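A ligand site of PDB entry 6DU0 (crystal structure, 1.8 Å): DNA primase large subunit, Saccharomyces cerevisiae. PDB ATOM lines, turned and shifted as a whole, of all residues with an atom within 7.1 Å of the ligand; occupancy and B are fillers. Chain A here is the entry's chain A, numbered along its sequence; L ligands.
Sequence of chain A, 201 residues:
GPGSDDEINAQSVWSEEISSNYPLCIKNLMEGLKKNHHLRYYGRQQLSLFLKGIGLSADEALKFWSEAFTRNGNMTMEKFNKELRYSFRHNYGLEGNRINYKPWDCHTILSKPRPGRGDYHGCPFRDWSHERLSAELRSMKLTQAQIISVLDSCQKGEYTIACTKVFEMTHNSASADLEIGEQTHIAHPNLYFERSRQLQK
The backbone carbonyl oxygen (O) of Ala 187 lies within hydrogen-bond range of the backbone NH (N) of Cys 106 (2.9 Å).
The backbone NH (N) of His 188 sits close to the side-chain sulfur (SG) of Cys 106 (3.1 Å).
The backbone NH (N) of Phe 125 lies close to the side-chain sulfur (SG) of Cys 123 (3.7 Å).
FE3 of the ligand is bound by SG of Cys 25 (2.3 Å).
An iron atom (FE4) of the ligand is bound by the side-chain sulfur (SG) of Cys 106.
SG of Cys 123 is bound to FE2 of the ligand (2.3 Å).
FE1 of the ligand is bound by SG of Cys 163, 2.2 Å away.
Residues that only touch the ligand: Phe 125 (3.7 Å), Pro 189 (3.7 Å) and Pro 23 (3.99 Å).
Hydrophobic or aromatic side chains that line the ligand: Pro 23, Phe 125 and Pro 189.
The nearest printed residue that does not touch the ligand is Ile 109 (4.2 Å).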
ATOM      1  N   PRO A  23     -19.683 -12.767  12.775  1.00  0.00           N
ATOM      2  CA  PRO A  23     -18.235 -12.803  12.690  1.00  0.00           C
ATOM      3  C   PRO A  23     -17.890 -14.164  12.060  1.00  0.00           C
ATOM      4  O   PRO A  23     -18.786 -14.917  11.774  1.00  0.00           O
ATOM      5  CB  PRO A  23     -17.815 -12.690  14.145  1.00  0.00           C
ATOM      6  CG  PRO A  23     -18.902 -13.430  14.887  1.00  0.00           C
ATOM      7  CD  PRO A  23     -20.167 -13.096  14.128  1.00  0.00           C
ATOM      8  N   LEU A  24     -16.609 -14.439  11.894  1.00  0.00           N
ATOM      9  CA  LEU A  24     -16.164 -15.515  11.018  1.00  0.00           C
ATOM     10  C   LEU A  24     -16.428 -16.892  11.658  1.00  0.00           C
ATOM     11  O   LEU A  24     -16.729 -17.837  10.933  1.00  0.00           O
ATOM     12  CB  LEU A  24     -14.684 -15.309  10.698  1.00  0.00           C
ATOM     13  CG  LEU A  24     -14.276 -15.516   9.248  1.00  0.00           C
ATOM     14  CD1 LEU A  24     -14.846 -14.411   8.365  1.00  0.00           C
ATOM     15  CD2 LEU A  24     -12.763 -15.546   9.114  1.00  0.00           C
ATOM     16  N   CYS A  25     -16.259 -17.007  12.987  1.00  0.00           N
ATOM     17  CA  CYS A  25     -16.538 -18.249  13.735  1.00  0.00           C
ATOM     18  C   CYS A  25     -17.988 -18.712  13.479  1.00  0.00           C
ATOM     19  O   CYS A  25     -18.206 -19.840  13.035  1.00  0.00           O
ATOM     20  CB  CYS A  25     -16.258 -18.082  15.224  1.00  0.00           C
ATOM     21  SG  CYS A  25     -17.149 -16.696  15.986  1.00  0.00           S
ATOM     22  N   ILE A  26     -18.950 -17.803  13.702  1.00  0.00           N
ATOM     23  CA  ILE A  26     -20.375 -18.080  13.478  1.00  0.00           C
ATOM     24  C   ILE A  26     -20.653 -18.447  12.010  1.00  0.00           C
ATOM     25  O   ILE A  26     -21.498 -19.285  11.766  1.00  0.00           O
ATOM     26  CB  ILE A  26     -21.251 -16.875  13.883  1.00  0.00           C
ATOM     27  CG1 ILE A  26     -21.169 -16.586  15.387  1.00  0.00           C
ATOM     28  CG2 ILE A  26     -22.683 -17.056  13.419  1.00  0.00           C
ATOM     29  CD1 ILE A  26     -21.409 -17.787  16.281  1.00  0.00           C
ATOM     30  N   GLN A  46     -21.510 -23.457  20.812  1.00  0.00           N
ATOM     31  CA  GLN A  46     -21.025 -22.154  20.342  1.00  0.00           C
ATOM     32  C   GLN A  46     -22.144 -21.496  19.528  1.00  0.00           C
ATOM     33  O   GLN A  46     -22.513 -20.321  19.786  1.00  0.00           O
ATOM     34  CB  GLN A  46     -19.750 -22.300  19.509  1.00  0.00           C
ATOM     35  CG  GLN A  46     -18.985 -20.989  19.300  1.00  0.00           C
ATOM     36  CD  GLN A  46     -17.605 -21.178  18.698  1.00  0.00           C
ATOM     37  OE1 GLN A  46     -16.989 -22.244  18.778  1.00  0.00           O
ATOM     38  NE2 GLN A  46     -17.110 -20.138  18.064  1.00  0.00           N
ATOM     39  N   ASP A 105     -18.053 -15.973  25.042  1.00  0.00           N
ATOM     40  CA  ASP A 105     -17.254 -14.807  24.658  1.00  0.00           C
ATOM     41  C   ASP A 105     -16.056 -15.308  23.849  1.00  0.00           C
ATOM     42  O   ASP A 105     -15.832 -16.531  23.757  1.00  0.00           O
ATOM     43  CB  ASP A 105     -16.832 -13.996  25.889  1.00  0.00           C
ATOM     44  CG  ASP A 105     -15.978 -14.752  26.884  1.00  0.00           C
ATOM     45  OD1 ASP A 105     -16.531 -15.637  27.573  1.00  0.00           O
ATOM     46  OD2 ASP A 105     -14.769 -14.475  26.938  1.00  0.00           O
ATOM     47  N   CYS A 106     -15.309 -14.357  23.273  1.00  0.00           N
ATOM     48  CA  CYS A 106     -14.121 -14.646  22.440  1.00  0.00           C
ATOM     49  C   CYS A 106     -13.065 -15.436  23.270  1.00  0.00           C
ATOM     50  O   CYS A 106     -12.446 -16.371  22.779  1.00  0.00           O
ATOM     51  CB  CYS A 106     -13.577 -13.360  21.801  1.00  0.00           C
ATOM     52  SG  CYS A 106     -14.674 -12.449  20.674  1.00  0.00           S
ATOM     53  N   HIS A 107     -12.880 -15.119  24.559  1.00  0.00           N
ATOM     54  CA  HIS A 107     -11.868 -15.810  25.424  1.00  0.00           C
ATOM     55  C   HIS A 107     -12.307 -17.245  25.742  1.00  0.00           C
ATOM     56  O   HIS A 107     -11.465 -18.153  25.832  1.00  0.00           O
ATOM     57  CB  HIS A 107     -11.616 -15.016  26.726  1.00  0.00           C
ATOM     58  CG  HIS A 107     -10.419 -15.463  27.488  1.00  0.00           C
ATOM     59  ND1 HIS A 107      -9.125 -15.174  27.081  1.00  0.00           N
ATOM     60  CD2 HIS A 107     -10.300 -16.165  28.642  1.00  0.00           C
ATOM     61  CE1 HIS A 107      -8.266 -15.681  27.947  1.00  0.00           C
ATOM     62  NE2 HIS A 107      -8.965 -16.289  28.914  1.00  0.00           N
ATOM     63  N   ILE A 109     -14.240 -19.049  23.761  1.00  0.00           N
ATOM     64  CA  ILE A 109     -14.228 -19.787  22.512  1.00  0.00           C
ATOM     65  C   ILE A 109     -12.807 -20.318  22.294  1.00  0.00           C
ATOM     66  O   ILE A 109     -12.640 -21.462  21.960  1.00  0.00           O
ATOM     67  CB  ILE A 109     -14.716 -18.932  21.314  1.00  0.00           C
ATOM     68  CG1 ILE A 109     -16.221 -18.693  21.400  1.00  0.00           C
ATOM     69  CG2 ILE A 109     -14.335 -19.571  19.972  1.00  0.00           C
ATOM     70  CD1 ILE A 109     -16.731 -17.595  20.501  1.00  0.00           C
ATOM     71  N   LEU A 110     -11.814 -19.455  22.484  1.00  0.00           N
ATOM     72  CA  LEU A 110     -10.396 -19.805  22.312  1.00  0.00           C
ATOM     73  C   LEU A 110      -9.956 -20.837  23.359  1.00  0.00           C
ATOM     74  O   LEU A 110      -9.182 -21.755  23.033  1.00  0.00           O
ATOM     75  CB  LEU A 110      -9.571 -18.511  22.386  1.00  0.00           C
ATOM     76  CG  LEU A 110      -9.754 -17.577  21.189  1.00  0.00           C
ATOM     77  CD1 LEU A 110      -9.405 -16.128  21.536  1.00  0.00           C
ATOM     78  CD2 LEU A 110      -8.915 -18.062  20.002  1.00  0.00           C
ATOM     79  N   GLY A 122     -14.569 -22.772  17.662  1.00  0.00           N
ATOM     80  CA  GLY A 122     -13.289 -22.074  17.890  1.00  0.00           C
ATOM     81  C   GLY A 122     -13.189 -20.847  17.017  1.00  0.00           C
ATOM     82  O   GLY A 122     -14.192 -20.328  16.584  1.00  0.00           O
ATOM     83  N   CYS A 123     -11.957 -20.415  16.700  1.00  0.00           N
ATOM     84  CA  CYS A 123     -11.772 -19.131  16.029  1.00  0.00           C
ATOM     85  C   CYS A 123     -10.942 -19.240  14.742  1.00  0.00           C
ATOM     86  O   CYS A 123      -9.748 -19.419  14.799  1.00  0.00           O
ATOM     87  CB  CYS A 123     -11.116 -18.131  16.965  1.00  0.00           C
ATOM     88  SG  CYS A 123     -10.747 -16.587  16.110  1.00  0.00           S
ATOM     89  N   PRO A 124     -11.565 -19.048  13.551  1.00  0.00           N
ATOM     90  CA  PRO A 124     -10.865 -19.139  12.264  1.00  0.00           C
ATOM     91  C   PRO A 124      -9.550 -18.359  12.105  1.00  0.00           C
ATOM     92  O   PRO A 124      -8.619 -18.856  11.435  1.00  0.00           O
ATOM     93  CB  PRO A 124     -11.879 -18.536  11.285  1.00  0.00           C
ATOM     94  CG  PRO A 124     -13.214 -18.884  11.892  1.00  0.00           C
ATOM     95  CD  PRO A 124     -13.000 -18.751  13.381  1.00  0.00           C
ATOM     96  N   PHE A 125      -9.473 -17.172  12.725  1.00  0.00           N
ATOM     97  CA  PHE A 125      -8.284 -16.327  12.724  1.00  0.00           C
ATOM     98  C   PHE A 125      -7.080 -17.045  13.333  1.00  0.00           C
ATOM     99  O   PHE A 125      -5.937 -16.744  12.961  1.00  0.00           O
ATOM    100  CB  PHE A 125      -8.547 -15.016  13.470  1.00  0.00           C
ATOM    101  CG  PHE A 125      -9.529 -14.116  12.758  1.00  0.00           C
ATOM    102  CD1 PHE A 125      -9.193 -13.524  11.552  1.00  0.00           C
ATOM    103  CD2 PHE A 125     -10.795 -13.906  13.275  1.00  0.00           C
ATOM    104  CE1 PHE A 125     -10.092 -12.695  10.895  1.00  0.00           C
ATOM    105  CE2 PHE A 125     -11.699 -13.090  12.615  1.00  0.00           C
ATOM    106  CZ  PHE A 125     -11.348 -12.492  11.428  1.00  0.00           C
ATOM    107  N   ARG A 126      -7.339 -17.944  14.289  1.00  0.00           N
ATOM    108  CA  ARG A 126      -6.328 -18.830  14.864  1.00  0.00           C
ATOM    109  C   ARG A 126      -6.312 -20.174  14.115  1.00  0.00           C
ATOM    110  O   ARG A 126      -5.266 -20.744  13.895  1.00  0.00           O
ATOM    111  CB  ARG A 126      -6.622 -19.031  16.348  1.00  0.00           C
ATOM    112  CG  ARG A 126      -5.532 -19.757  17.136  1.00  0.00           C
ATOM    113  CD  ARG A 126      -5.820 -21.217  17.363  1.00  0.00           C
ATOM    114  NE  ARG A 126      -7.046 -21.407  18.126  1.00  0.00           N
ATOM    115  CZ  ARG A 126      -7.127 -21.342  19.451  1.00  0.00           C
ATOM    116  NH1 ARG A 126      -6.042 -21.114  20.174  1.00  0.00           N
ATOM    117  NH2 ARG A 126      -8.299 -21.500  20.044  1.00  0.00           N
ATOM    118  N   TYR A 159      -6.035 -12.514  17.704  1.00  0.00           N
ATOM    119  CA  TYR A 159      -7.184 -12.915  16.928  1.00  0.00           C
ATOM    120  C   TYR A 159      -8.327 -11.928  17.108  1.00  0.00           C
ATOM    121  O   TYR A 159      -8.977 -11.560  16.126  1.00  0.00           O
ATOM    122  CB  TYR A 159      -7.582 -14.347  17.298  1.00  0.00           C
ATOM    123  CG  TYR A 159      -6.393 -15.263  17.335  1.00  0.00           C
ATOM    124  CD1 TYR A 159      -5.560 -15.346  16.235  1.00  0.00           C
ATOM    125  CD2 TYR A 159      -6.048 -15.967  18.476  1.00  0.00           C
ATOM    126  CE1 TYR A 159      -4.434 -16.161  16.257  1.00  0.00           C
ATOM    127  CE2 TYR A 159      -4.922 -16.770  18.516  1.00  0.00           C
ATOM    128  CZ  TYR A 159      -4.111 -16.871  17.396  1.00  0.00           C
ATOM    129  OH  TYR A 159      -3.015 -17.668  17.393  1.00  0.00           O
ATOM    130  N   THR A 160      -8.551 -11.461  18.338  1.00  0.00           N
ATOM    131  CA  THR A 160      -9.586 -10.460  18.572  1.00  0.00           C
ATOM    132  C   THR A 160      -9.296  -9.189  17.767  1.00  0.00           C
ATOM    133  O   THR A 160     -10.224  -8.524  17.342  1.00  0.00           O
ATOM    134  CB  THR A 160      -9.748 -10.166  20.075  1.00  0.00           C
ATOM    135  OG1 THR A 160      -8.511  -9.637  20.554  1.00  0.00           O
ATOM    136  CG2 THR A 160     -10.151 -11.394  20.868  1.00  0.00           C
ATOM    137  N   ILE A 161      -8.018  -8.859  17.552  1.00  0.00           N
ATOM    138  CA  ILE A 161      -7.621  -7.660  16.762  1.00  0.00           C
ATOM    139  C   ILE A 161      -7.880  -7.952  15.265  1.00  0.00           C
ATOM    140  O   ILE A 161      -8.465  -7.138  14.548  1.00  0.00           O
ATOM    141  CB  ILE A 161      -6.142  -7.260  16.996  1.00  0.00           C
ATOM    142  CG1 ILE A 161      -5.802  -7.056  18.479  1.00  0.00           C
ATOM    143  CG2 ILE A 161      -5.788  -6.029  16.172  1.00  0.00           C
ATOM    144  CD1 ILE A 161      -6.435  -5.838  19.119  1.00  0.00           C
ATOM    145  N   ALA A 162      -7.419  -9.126  14.826  1.00  0.00           N
ATOM    146  CA  ALA A 162      -7.647  -9.615  13.472  1.00  0.00           C
ATOM    147  C   ALA A 162      -9.145  -9.501  13.131  1.00  0.00           C
ATOM    148  O   ALA A 162      -9.540  -8.890  12.142  1.00  0.00           O
ATOM    149  CB  ALA A 162      -7.153 -11.029  13.355  1.00  0.00           C
ATOM    150  N   CYS A 163      -9.978 -10.050  14.018  1.00  0.00           N
ATOM    151  CA  CYS A 163     -11.430 -10.013  13.854  1.00  0.00           C
ATOM    152  C   CYS A 163     -11.943  -8.565  13.834  1.00  0.00           C
ATOM    153  O   CYS A 163     -12.713  -8.215  12.930  1.00  0.00           O
ATOM    154  CB  CYS A 163     -12.084 -10.829  14.951  1.00  0.00           C
ATOM    155  SG  CYS A 163     -13.854 -11.057  14.683  1.00  0.00           S
ATOM    156  N   THR A 164     -11.538  -7.725  14.788  1.00  0.00           N
ATOM    157  CA  THR A 164     -11.988  -6.307  14.829  1.00  0.00           C
ATOM    158  C   THR A 164     -11.597  -5.597  13.530  1.00  0.00           C
ATOM    159  O   THR A 164     -12.315  -4.723  13.048  1.00  0.00           O
ATOM    160  CB  THR A 164     -11.387  -5.514  15.992  1.00  0.00           C
ATOM    161  OG1 THR A 164     -11.590  -6.222  17.215  1.00  0.00           O
ATOM    162  CG2 THR A 164     -11.974  -4.112  16.098  1.00  0.00           C
ATOM    163  N   ALA A 187     -14.573  -8.348  24.117  1.00  0.00           N
ATOM    164  CA  ALA A 187     -14.338  -9.301  22.948  1.00  0.00           C
ATOM    165  C   ALA A 187     -15.383 -10.437  22.917  1.00  0.00           C
ATOM    166  O   ALA A 187     -15.228 -11.430  23.627  1.00  0.00           O
ATOM    167  CB  ALA A 187     -12.948  -9.856  23.014  1.00  0.00           C
ATOM    168  N   HIS A 188     -16.430 -10.265  22.101  1.00  0.00           N
ATOM    169  CA  HIS A 188     -17.654 -11.092  22.170  1.00  0.00           C
ATOM    170  C   HIS A 188     -18.337 -11.193  20.806  1.00  0.00           C
ATOM    171  O   HIS A 188     -18.756 -10.188  20.225  1.00  0.00           O
ATOM    172  CB  HIS A 188     -18.599 -10.555  23.244  1.00  0.00           C
ATOM    173  CG  HIS A 188     -19.523 -11.595  23.787  1.00  0.00           C
ATOM    174  ND1 HIS A 188     -20.527 -12.156  23.026  1.00  0.00           N
ATOM    175  CD2 HIS A 188     -19.549 -12.226  24.986  1.00  0.00           C
ATOM    176  CE1 HIS A 188     -21.157 -13.075  23.746  1.00  0.00           C
ATOM    177  NE2 HIS A 188     -20.564 -13.147  24.948  1.00  0.00           N
ATOM    178  N   PRO A 189     -18.525 -12.421  20.248  1.00  0.00           N
ATOM    179  CA  PRO A 189     -19.162 -12.575  18.932  1.00  0.00           C
ATOM    180  C   PRO A 189     -20.549 -11.926  18.856  1.00  0.00           C
ATOM    181  O   PRO A 189     -20.917 -11.383  17.832  1.00  0.00           O
ATOM    182  CB  PRO A 189     -19.276 -14.098  18.722  1.00  0.00           C
ATOM    183  CG  PRO A 189     -18.298 -14.697  19.712  1.00  0.00           C
ATOM    184  CD  PRO A 189     -18.248 -13.725  20.867  1.00  0.00           C
ATOM    185  N   ASN A 190     -21.320 -11.977  19.945  1.00  0.00           N
ATOM    186  CA  ASN A 190     -22.619 -11.347  20.020  1.00  0.00           C
ATOM    187  C   ASN A 190     -22.469  -9.819  19.996  1.00  0.00           C
ATOM    188  O   ASN A 190     -23.348  -9.126  19.516  1.00  0.00           O
ATOM    189  CB  ASN A 190     -23.390 -11.840  21.247  1.00  0.00           C
ATOM    190  CG  ASN A 190     -23.887 -13.259  21.079  1.00  0.00           C
ATOM    191  OD1 ASN A 190     -23.239 -14.210  21.508  1.00  0.00           O
ATOM    192  ND2 ASN A 190     -25.022 -13.400  20.426  1.00  0.00           N
ATOM    193  N   TYR A 192     -19.936  -8.459  18.239  1.00  0.00           N
ATOM    194  CA  TYR A 192     -19.679  -8.359  16.794  1.00  0.00           C
ATOM    195  C   TYR A 192     -21.011  -8.197  16.073  1.00  0.00           C
ATOM    196  O   TYR A 192     -21.142  -7.372  15.158  1.00  0.00           O
ATOM    197  CB  TYR A 192     -18.936  -9.588  16.245  1.00  0.00           C
ATOM    198  CG  TYR A 192     -18.329  -9.425  14.867  1.00  0.00           C
ATOM    199  CD1 TYR A 192     -19.127  -9.378  13.729  1.00  0.00           C
ATOM    200  CD2 TYR A 192     -16.964  -9.329  14.693  1.00  0.00           C
ATOM    201  CE1 TYR A 192     -18.573  -9.223  12.467  1.00  0.00           C
ATOM    202  CE2 TYR A 192     -16.394  -9.198  13.436  1.00  0.00           C
ATOM    203  CZ  TYR A 192     -17.201  -9.143  12.319  1.00  0.00           C
ATOM    204  OH  TYR A 192     -16.639  -9.004  11.084  1.00  0.00           O
HETATM  205 FE1  LIG L   1     -14.227 -12.760  16.096  1.00  0.00          FE
HETATM  206 FE2  LIG L   1     -12.461 -15.189  16.638  1.00  0.00          FE
HETATM  207 FE3  LIG L   1     -15.315 -15.425  16.464  1.00  0.00          FE
HETATM  208 FE4  LIG L   1     -14.197 -13.895  18.868  1.00  0.00          FE
HETATM  209  S1  LIG L   1     -13.881 -15.916  17.865  1.00  0.00           S
HETATM  210  S2  LIG L   1     -15.658 -13.475  17.411  1.00  0.00           S
HETATM  211  S3  LIG L   1     -12.797 -13.194  17.577  1.00  0.00           S
HETATM  212  S4  LIG L   1     -13.867 -14.713  15.124  1.00  0.00           S
